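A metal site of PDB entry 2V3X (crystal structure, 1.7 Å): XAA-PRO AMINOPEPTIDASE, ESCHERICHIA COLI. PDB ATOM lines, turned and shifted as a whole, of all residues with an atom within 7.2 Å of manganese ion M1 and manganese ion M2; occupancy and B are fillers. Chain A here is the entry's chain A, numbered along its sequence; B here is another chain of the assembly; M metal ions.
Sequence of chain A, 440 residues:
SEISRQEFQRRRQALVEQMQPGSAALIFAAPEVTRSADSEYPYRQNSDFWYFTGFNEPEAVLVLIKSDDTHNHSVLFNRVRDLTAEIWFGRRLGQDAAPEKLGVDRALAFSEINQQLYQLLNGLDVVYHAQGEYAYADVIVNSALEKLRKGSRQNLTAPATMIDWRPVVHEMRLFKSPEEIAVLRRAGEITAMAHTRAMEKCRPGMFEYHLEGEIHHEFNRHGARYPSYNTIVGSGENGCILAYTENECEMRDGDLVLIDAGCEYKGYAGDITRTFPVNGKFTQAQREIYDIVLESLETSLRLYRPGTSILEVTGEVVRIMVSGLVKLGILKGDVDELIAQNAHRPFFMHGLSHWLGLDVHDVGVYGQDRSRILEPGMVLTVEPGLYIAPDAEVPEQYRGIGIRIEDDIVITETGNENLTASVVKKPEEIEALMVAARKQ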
ATOM      1  N   TYR A 229     -23.023 -12.809 -27.961  1.00  0.00           N
ATOM      2  CA  TYR A 229     -22.934 -13.934 -27.045  1.00  0.00           C
ATOM      3  C   TYR A 229     -24.236 -14.694 -27.130  1.00  0.00           C
ATOM      4  O   TYR A 229     -25.219 -14.178 -27.661  1.00  0.00           O
ATOM      5  CB  TYR A 229     -22.673 -13.496 -25.611  1.00  0.00           C
ATOM      6  CG  TYR A 229     -23.640 -12.496 -25.093  1.00  0.00           C
ATOM      7  CD1 TYR A 229     -23.441 -11.149 -25.321  1.00  0.00           C
ATOM      8  CD2 TYR A 229     -24.785 -12.875 -24.390  1.00  0.00           C
ATOM      9  CE1 TYR A 229     -24.340 -10.207 -24.880  1.00  0.00           C
ATOM     10  CE2 TYR A 229     -25.681 -11.933 -23.906  1.00  0.00           C
ATOM     11  CZ  TYR A 229     -25.456 -10.591 -24.164  1.00  0.00           C
ATOM     12  OH  TYR A 229     -26.327  -9.602 -23.734  1.00  0.00           O
ATOM     13  N   ILE A 232     -29.699 -15.326 -23.571  1.00  0.00           N
ATOM     14  CA  ILE A 232     -30.263 -15.916 -22.337  1.00  0.00           C
ATOM     15  C   ILE A 232     -31.721 -15.449 -22.232  1.00  0.00           C
ATOM     16  O   ILE A 232     -31.997 -14.247 -22.224  1.00  0.00           O
ATOM     17  CB  ILE A 232     -29.458 -15.391 -21.122  1.00  0.00           C
ATOM     18  CG1 ILE A 232     -28.021 -15.916 -21.182  1.00  0.00           C
ATOM     19  CG2 ILE A 232     -30.131 -15.717 -19.798  1.00  0.00           C
ATOM     20  CD1 ILE A 232     -27.016 -15.022 -20.482  1.00  0.00           C
ATOM     21  N   ILE A 259     -34.117 -11.531 -19.788  1.00  0.00           N
ATOM     22  CA  ILE A 259     -33.513 -11.633 -21.118  1.00  0.00           C
ATOM     23  C   ILE A 259     -32.186 -10.890 -21.103  1.00  0.00           C
ATOM     24  O   ILE A 259     -32.157  -9.693 -20.852  1.00  0.00           O
ATOM     25  CB  ILE A 259     -34.405 -11.065 -22.181  1.00  0.00           C
ATOM     26  CG1 ILE A 259     -35.730 -11.831 -22.246  1.00  0.00           C
ATOM     27  CG2 ILE A 259     -33.726 -11.149 -23.542  1.00  0.00           C
ATOM     28  CD1 ILE A 259     -36.631 -11.373 -23.392  1.00  0.00           C
ATOM     29  N   ASP A 260     -31.106 -11.612 -21.352  1.00  0.00           N
ATOM     30  CA  ASP A 260     -29.764 -11.023 -21.473  1.00  0.00           C
ATOM     31  C   ASP A 260     -29.329 -11.315 -22.908  1.00  0.00           C
ATOM     32  O   ASP A 260     -29.145 -12.474 -23.299  1.00  0.00           O
ATOM     33  CB  ASP A 260     -28.831 -11.647 -20.445  1.00  0.00           C
ATOM     34  CG  ASP A 260     -27.502 -10.894 -20.281  1.00  0.00           C
ATOM     35  OD1 ASP A 260     -27.114 -10.138 -21.175  1.00  0.00           O
ATOM     36  OD2 ASP A 260     -26.854 -11.057 -19.229  1.00  0.00           O
ATOM     37  N   ALA A 261     -29.267 -10.271 -23.731  1.00  0.00           N
ATOM     38  CA  ALA A 261     -28.984 -10.419 -25.149  1.00  0.00           C
ATOM     39  C   ALA A 261     -28.317  -9.181 -25.672  1.00  0.00           C
ATOM     40  O   ALA A 261     -28.614  -8.060 -25.241  1.00  0.00           O
ATOM     41  CB  ALA A 261     -30.286 -10.693 -25.955  1.00  0.00           C
ATOM     42  N   GLY A 262     -27.436  -9.396 -26.633  1.00  0.00           N
ATOM     43  CA  GLY A 262     -26.694  -8.306 -27.241  1.00  0.00           C
ATOM     44  C   GLY A 262     -26.278  -8.628 -28.661  1.00  0.00           C
ATOM     45  O   GLY A 262     -25.982  -9.771 -28.997  1.00  0.00           O
ATOM     46  N   GLY A 270     -23.129  -5.089 -28.094  1.00  0.00           N
ATOM     47  CA  GLY A 270     -24.110  -4.605 -27.130  1.00  0.00           C
ATOM     48  C   GLY A 270     -24.317  -5.675 -26.067  1.00  0.00           C
ATOM     49  O   GLY A 270     -23.978  -6.872 -26.262  1.00  0.00           O
ATOM     50  N   ASP A 271     -24.879  -5.275 -24.936  1.00  0.00           N
ATOM     51  CA  ASP A 271     -25.099  -6.204 -23.826  1.00  0.00           C
ATOM     52  C   ASP A 271     -26.143  -5.625 -22.906  1.00  0.00           C
ATOM     53  O   ASP A 271     -25.835  -4.841 -22.022  1.00  0.00           O
ATOM     54  CB  ASP A 271     -23.772  -6.482 -23.112  1.00  0.00           C
ATOM     55  CG  ASP A 271     -23.889  -7.466 -21.970  1.00  0.00           C
ATOM     56  OD1 ASP A 271     -24.954  -8.077 -21.763  1.00  0.00           O
ATOM     57  OD2 ASP A 271     -22.877  -7.663 -21.277  1.00  0.00           O
ATOM     58  N   ILE A 272     -27.398  -6.021 -23.102  1.00  0.00           N
ATOM     59  CA  ILE A 272     -28.501  -5.501 -22.290  1.00  0.00           C
ATOM     60  C   ILE A 272     -29.188  -6.666 -21.568  1.00  0.00           C
ATOM     61  O   ILE A 272     -29.363  -7.738 -22.155  1.00  0.00           O
ATOM     62  CB  ILE A 272     -29.517  -4.747 -23.144  1.00  0.00           C
ATOM     63  CG1 ILE A 272     -28.936  -3.444 -23.726  1.00  0.00           C
ATOM     64  CG2 ILE A 272     -30.849  -4.465 -22.362  1.00  0.00           C
ATOM     65  CD1 ILE A 272     -29.945  -2.681 -24.629  1.00  0.00           C
ATOM     66  N   THR A 273     -29.592  -6.443 -20.323  1.00  0.00           N
ATOM     67  CA  THR A 273     -30.515  -7.355 -19.647  1.00  0.00           C
ATOM     68  C   THR A 273     -31.753  -6.571 -19.212  1.00  0.00           C
ATOM     69  O   THR A 273     -31.655  -5.452 -18.674  1.00  0.00           O
ATOM     70  CB  THR A 273     -29.916  -8.049 -18.393  1.00  0.00           C
ATOM     71  OG1 THR A 273     -28.650  -8.648 -18.712  1.00  0.00           O
ATOM     72  CG2 THR A 273     -30.868  -9.161 -17.858  1.00  0.00           C
ATOM     73  N   LEU A 352     -20.621  -6.224 -10.602  1.00  0.00           N
ATOM     74  CA  LEU A 352     -21.535  -5.167 -11.079  1.00  0.00           C
ATOM     75  C   LEU A 352     -21.290  -4.753 -12.526  1.00  0.00           C
ATOM     76  O   LEU A 352     -22.220  -4.311 -13.226  1.00  0.00           O
ATOM     77  CB  LEU A 352     -21.399  -3.927 -10.179  1.00  0.00           C
ATOM     78  CG  LEU A 352     -22.287  -2.706 -10.457  1.00  0.00           C
ATOM     79  CD1 LEU A 352     -23.782  -3.081 -10.237  1.00  0.00           C
ATOM     80  CD2 LEU A 352     -21.902  -1.527  -9.582  1.00  0.00           C
ATOM     81  N   SER A 353     -20.031  -4.826 -12.963  1.00  0.00           N
ATOM     82  CA  SER A 353     -19.621  -4.227 -14.227  1.00  0.00           C
ATOM     83  C   SER A 353     -18.480  -4.966 -14.849  1.00  0.00           C
ATOM     84  O   SER A 353     -17.543  -5.388 -14.158  1.00  0.00           O
ATOM     85  CB  SER A 353     -19.157  -2.776 -13.984  1.00  0.00           C
ATOM     86  OG  SER A 353     -20.246  -1.950 -13.544  1.00  0.00           O
ATOM     87  N   HIS A 354     -18.531  -5.067 -16.166  1.00  0.00           N
ATOM     88  CA  HIS A 354     -17.386  -5.511 -16.951  1.00  0.00           C
ATOM     89  C   HIS A 354     -17.155  -4.561 -18.121  1.00  0.00           C
ATOM     90  O   HIS A 354     -18.084  -3.910 -18.613  1.00  0.00           O
ATOM     91  CB  HIS A 354     -17.545  -6.956 -17.465  1.00  0.00           C
ATOM     92  CG  HIS A 354     -18.769  -7.206 -18.286  1.00  0.00           C
ATOM     93  ND1 HIS A 354     -18.840  -6.916 -19.643  1.00  0.00           N
ATOM     94  CD2 HIS A 354     -19.955  -7.750 -17.942  1.00  0.00           C
ATOM     95  CE1 HIS A 354     -20.048  -7.243 -20.076  1.00  0.00           C
ATOM     96  NE2 HIS A 354     -20.743  -7.754 -19.064  1.00  0.00           N
ATOM     97  N   TRP A 355     -15.915  -4.495 -18.584  1.00  0.00           N
ATOM     98  CA  TRP A 355     -15.605  -3.762 -19.796  1.00  0.00           C
ATOM     99  C   TRP A 355     -16.369  -4.320 -20.996  1.00  0.00           C
ATOM    100  O   TRP A 355     -16.700  -5.507 -21.044  1.00  0.00           O
ATOM    101  CB  TRP A 355     -14.115  -3.839 -20.136  1.00  0.00           C
ATOM    102  CG  TRP A 355     -13.131  -3.553 -19.062  1.00  0.00           C
ATOM    103  CD1 TRP A 355     -12.082  -4.325 -18.713  1.00  0.00           C
ATOM    104  CD2 TRP A 355     -13.050  -2.377 -18.213  1.00  0.00           C
ATOM    105  NE1 TRP A 355     -11.336  -3.731 -17.723  1.00  0.00           N
ATOM    106  CE2 TRP A 355     -11.923  -2.547 -17.382  1.00  0.00           C
ATOM    107  CE3 TRP A 355     -13.814  -1.217 -18.091  1.00  0.00           C
ATOM    108  CZ2 TRP A 355     -11.531  -1.602 -16.437  1.00  0.00           C
ATOM    109  CZ3 TRP A 355     -13.423  -0.275 -17.133  1.00  0.00           C
ATOM    110  CH2 TRP A 355     -12.294  -0.474 -16.322  1.00  0.00           C
ATOM    111  N   LEU A 356     -16.626  -3.464 -21.976  1.00  0.00           N
ATOM    112  CA  LEU A 356     -17.390  -3.845 -23.164  1.00  0.00           C
ATOM    113  C   LEU A 356     -16.656  -3.309 -24.402  1.00  0.00           C
ATOM    114  O   LEU A 356     -16.154  -2.167 -24.398  1.00  0.00           O
ATOM    115  CB  LEU A 356     -18.797  -3.239 -23.077  1.00  0.00           C
ATOM    116  CG  LEU A 356     -19.848  -3.578 -24.135  1.00  0.00           C
ATOM    117  CD1 LEU A 356     -20.251  -5.047 -24.039  1.00  0.00           C
ATOM    118  CD2 LEU A 356     -21.061  -2.667 -23.953  1.00  0.00           C
ATOM    119  N   VAL A 360     -17.651  -9.075 -25.562  1.00  0.00           N
ATOM    120  CA  VAL A 360     -18.648  -8.711 -24.539  1.00  0.00           C
ATOM    121  C   VAL A 360     -18.022  -8.581 -23.164  1.00  0.00           C
ATOM    122  O   VAL A 360     -18.306  -7.611 -22.455  1.00  0.00           O
ATOM    123  CB  VAL A 360     -19.890  -9.653 -24.542  1.00  0.00           C
ATOM    124  CG1 VAL A 360     -19.549 -11.070 -24.243  1.00  0.00           C
ATOM    125  CG2 VAL A 360     -20.952  -9.086 -23.581  1.00  0.00           C
ATOM    126  N   HIS A 361     -17.160  -9.525 -22.778  1.00  0.00           N
ATOM    127  CA  HIS A 361     -16.325  -9.356 -21.588  1.00  0.00           C
ATOM    128  C   HIS A 361     -14.975  -8.848 -22.091  1.00  0.00           C
ATOM    129  O   HIS A 361     -14.064  -9.638 -22.438  1.00  0.00           O
ATOM    130  CB  HIS A 361     -16.159 -10.648 -20.820  1.00  0.00           C
ATOM    131  CG  HIS A 361     -17.433 -11.126 -20.214  1.00  0.00           C
ATOM    132  ND1 HIS A 361     -17.584 -12.424 -19.763  1.00  0.00           N
ATOM    133  CD2 HIS A 361     -18.609 -10.511 -19.991  1.00  0.00           C
ATOM    134  CE1 HIS A 361     -18.805 -12.563 -19.259  1.00  0.00           C
ATOM    135  NE2 HIS A 361     -19.451 -11.419 -19.393  1.00  0.00           N
ATOM    136  N   THR A 381     -20.387  -2.248 -18.611  1.00  0.00           N
ATOM    137  CA  THR A 381     -21.773  -2.554 -18.279  1.00  0.00           C
ATOM    138  C   THR A 381     -22.064  -2.217 -16.832  1.00  0.00           C
ATOM    139  O   THR A 381     -21.153  -2.064 -16.000  1.00  0.00           O
ATOM    140  CB  THR A 381     -22.084  -4.030 -18.518  1.00  0.00           C
ATOM    141  OG1 THR A 381     -21.341  -4.827 -17.576  1.00  0.00           O
ATOM    142  CG2 THR A 381     -21.779  -4.440 -19.967  1.00  0.00           C
ATOM    143  N   VAL A 382     -23.358  -2.111 -16.511  1.00  0.00           N
ATOM    144  CA  VAL A 382     -23.816  -1.927 -15.145  1.00  0.00           C
ATOM    145  C   VAL A 382     -24.962  -2.899 -14.966  1.00  0.00           C
ATOM    146  O   VAL A 382     -25.995  -2.731 -15.593  1.00  0.00           O
ATOM    147  CB  VAL A 382     -24.287  -0.497 -14.876  1.00  0.00           C
ATOM    148  CG1 VAL A 382     -24.564  -0.285 -13.356  1.00  0.00           C
ATOM    149  CG2 VAL A 382     -23.250   0.510 -15.413  1.00  0.00           C
ATOM    150  N   GLU A 383     -24.756  -3.926 -14.164  1.00  0.00           N
ATOM    151  CA  GLU A 383     -25.680  -5.078 -14.175  1.00  0.00           C
ATOM    152  C   GLU A 383     -25.936  -5.683 -12.802  1.00  0.00           C
ATOM    153  O   GLU A 383     -25.671  -6.867 -12.581  1.00  0.00           O
ATOM    154  CB  GLU A 383     -25.225  -6.146 -15.174  1.00  0.00           C
ATOM    155  CG  GLU A 383     -23.844  -6.722 -15.007  1.00  0.00           C
ATOM    156  CD  GLU A 383     -23.531  -7.678 -16.163  1.00  0.00           C
ATOM    157  OE1 GLU A 383     -24.279  -8.649 -16.370  1.00  0.00           O
ATOM    158  OE2 GLU A 383     -22.573  -7.386 -16.896  1.00  0.00           O
ATOM    159  N   ARG A 404     -32.300  -9.315 -13.178  1.00  0.00           N
ATOM    160  CA  ARG A 404     -31.125  -8.531 -13.518  1.00  0.00           C
ATOM    161  C   ARG A 404     -31.537  -7.430 -14.472  1.00  0.00           C
ATOM    162  O   ARG A 404     -32.412  -7.615 -15.332  1.00  0.00           O
ATOM    163  CB  ARG A 404     -30.036  -9.421 -14.161  1.00  0.00           C
ATOM    164  CG  ARG A 404     -28.797  -8.661 -14.615  1.00  0.00           C
ATOM    165  CD  ARG A 404     -27.597  -9.563 -14.904  1.00  0.00           C
ATOM    166  NE  ARG A 404     -27.743 -10.473 -16.040  1.00  0.00           N
ATOM    167  CZ  ARG A 404     -28.007 -11.797 -15.967  1.00  0.00           C
ATOM    168  NH1 ARG A 404     -28.239 -12.406 -14.812  1.00  0.00           N
ATOM    169  NH2 ARG A 404     -28.052 -12.536 -17.069  1.00  0.00           N
ATOM    170  N   GLU A 406     -29.571  -4.421 -16.831  1.00  0.00           N
ATOM    171  CA  GLU A 406     -28.211  -4.095 -17.297  1.00  0.00           C
ATOM    172  C   GLU A 406     -28.260  -3.087 -18.413  1.00  0.00           C
ATOM    173  O   GLU A 406     -28.969  -3.289 -19.421  1.00  0.00           O
ATOM    174  CB  GLU A 406     -27.545  -5.367 -17.796  1.00  0.00           C
ATOM    175  CG  GLU A 406     -26.212  -5.155 -18.535  1.00  0.00           C
ATOM    176  CD  GLU A 406     -25.561  -6.450 -18.909  1.00  0.00           C
ATOM    177  OE1 GLU A 406     -26.268  -7.458 -19.182  1.00  0.00           O
ATOM    178  OE2 GLU A 406     -24.316  -6.480 -18.936  1.00  0.00           O
ATOM    179  N   ASP A 407     -27.447  -2.044 -18.254  1.00  0.00           N
ATOM    180  CA  ASP A 407     -27.211  -0.989 -19.262  1.00  0.00           C
ATOM    181  C   ASP A 407     -25.707  -0.963 -19.592  1.00  0.00           C
ATOM    182  O   ASP A 407     -24.873  -1.478 -18.830  1.00  0.00           O
ATOM    183  CB  ASP A 407     -27.659   0.376 -18.761  1.00  0.00           C
ATOM    184  CG  ASP A 407     -29.189   0.628 -18.939  1.00  0.00           C
ATOM    185  OD1 ASP A 407     -29.824  -0.018 -19.824  1.00  0.00           O
ATOM    186  OD2 ASP A 407     -29.707   1.497 -18.206  1.00  0.00           O
ATOM    187  N   ASP A 408     -25.418  -0.396 -20.771  1.00  0.00           N
ATOM    188  CA  ASP A 408     -24.050  -0.177 -21.225  1.00  0.00           C
ATOM    189  C   ASP A 408     -23.778   1.326 -21.212  1.00  0.00           C
ATOM    190  O   ASP A 408     -24.590   2.106 -21.716  1.00  0.00           O
ATOM    191  CB  ASP A 408     -23.886  -0.687 -22.649  1.00  0.00           C
ATOM    192  CG  ASP A 408     -24.318  -2.138 -22.811  1.00  0.00           C
ATOM    193  OD1 ASP A 408     -24.204  -2.897 -21.824  1.00  0.00           O
ATOM    194  OD2 ASP A 408     -24.740  -2.508 -23.941  1.00  0.00           O
ATOM    195  N   VAL B   1     -24.116 -10.818 -20.816  1.00  0.00           N
ATOM    196  CA  VAL B   1     -23.910 -11.993 -19.911  1.00  0.00           C
ATOM    197  C   VAL B   1     -22.971 -11.634 -18.726  1.00  0.00           C
ATOM    198  O   VAL B   1     -21.961 -11.009 -18.930  1.00  0.00           O
ATOM    199  CB  VAL B   1     -23.383 -13.185 -20.719  1.00  0.00           C
ATOM    200  CG1 VAL B   1     -22.121 -12.808 -21.493  1.00  0.00           C
ATOM    201  CG2 VAL B   1     -23.168 -14.406 -19.824  1.00  0.00           C
ATOM    202  N   PRO B   2     -23.315 -12.027 -17.464  1.00  0.00           N
ATOM    203  CA  PRO B   2     -22.515 -11.613 -16.290  1.00  0.00           C
ATOM    204  C   PRO B   2     -21.064 -12.096 -16.224  1.00  0.00           C
ATOM    205  O   PRO B   2     -20.731 -13.166 -16.752  1.00  0.00           O
ATOM    206  CB  PRO B   2     -23.299 -12.182 -15.104  1.00  0.00           C
ATOM    207  CG  PRO B   2     -24.669 -12.370 -15.622  1.00  0.00           C
ATOM    208  CD  PRO B   2     -24.505 -12.790 -17.047  1.00  0.00           C
ATOM    209  N   LEU B   3     -20.228 -11.299 -15.548  1.00  0.00           N
ATOM    210  CA  LEU B   3     -18.833 -11.656 -15.243  1.00  0.00           C
ATOM    211  C   LEU B   3     -18.648 -11.700 -13.719  1.00  0.00           C
ATOM    212  O   LEU B   3     -18.106 -12.652 -13.157  1.00  0.00           O
ATOM    213  CB  LEU B   3     -17.869 -10.639 -15.873  1.00  0.00           C
ATOM    214  CG  LEU B   3     -16.375 -10.914 -15.722  1.00  0.00           C
ATOM    215  CD1 LEU B   3     -15.989 -12.203 -16.424  1.00  0.00           C
ATOM    216  CD2 LEU B   3     -15.525  -9.774 -16.229  1.00  0.00           C
ATOM    217  OXT LEU B   3     -19.037 -10.797 -12.998  1.00  0.00           O
HETATM  218 MN    MN M   1     -25.452  -9.185 -20.133  1.00  0.00          MN
HETATM  219 MN    MN M   2     -22.890  -7.967 -19.133  1.00  0.00          MN
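The backbone NH of Asp 271 sits at hydrogen-bond distance from the side-chain carboxylate of Asp 408 (2.9 Å).
ND1 of His 354 is in hydrogen-bond range of O of Val 360 (2.9 Å).
The side-chain hydroxyl of Thr 273 lies close to the side-chain carboxylate of Asp 260, at 3.0 Å.
OH of Tyr 229 lies close to OD1 of Asp 260 (2.7 Å).
O of Ile 232 lies within hydrogen-bond range of N of Asp 260, at 2.9 Å.
The backbone carbonyl oxygen (O) of Val 1 of chain B lies within hydrogen-bond range of a ring nitrogen (NE2) of His 361.
The side-chain hydroxyl (OG1) of Thr 273 is in hydrogen-bond range of the guanidinium group (NE) of Arg 404, 3.4 Å away.
The side-chain hydroxyl (OH) of Tyr 229 sits close to the backbone NH (N) of Ala 261 (3.0 Å).
OH of Tyr 229 touches manganese ion M1 (3.7 Å).
Thr 273 touches manganese ion M1.
Within 4 Å of manganese ion M1: Tyr 229, Asp 260, Asp 271, Thr 273, Glu 383, Glu 406 and Val 1 of chain B.
Merely in contact with manganese ion M2: Thr 381.
Six residues have an atom within 4 Å of manganese ion M2: Asp 271, His 354, Thr 381, Glu 383, Glu 406 and Val 1 of chain B.
Manganese ion M1 is bound by the side-chain carboxylate (OD1) of Asp 271 (2.0 Å), the side-chain carboxylate (OE1) of Glu 406 (2.1 Å), the side-chain carboxylate (OD1) of Asp 260 (2.2 Å), the backbone nitrogen (N) of Val 1 of chain B (2.2 Å) and the side-chain carboxylate (OD2) of Asp 260 (2.5 Å).
Manganese ion M2 is bound by the side-chain carboxylate (OE2) of Glu 406 (2.1 Å), a ring nitrogen (NE2) of His 354 (2.2 Å), the side-chain carboxylate (OD2) of Asp 271 (2.2 Å) and the side-chain carboxylate (OE2) of Glu 383 (2.3 Å).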
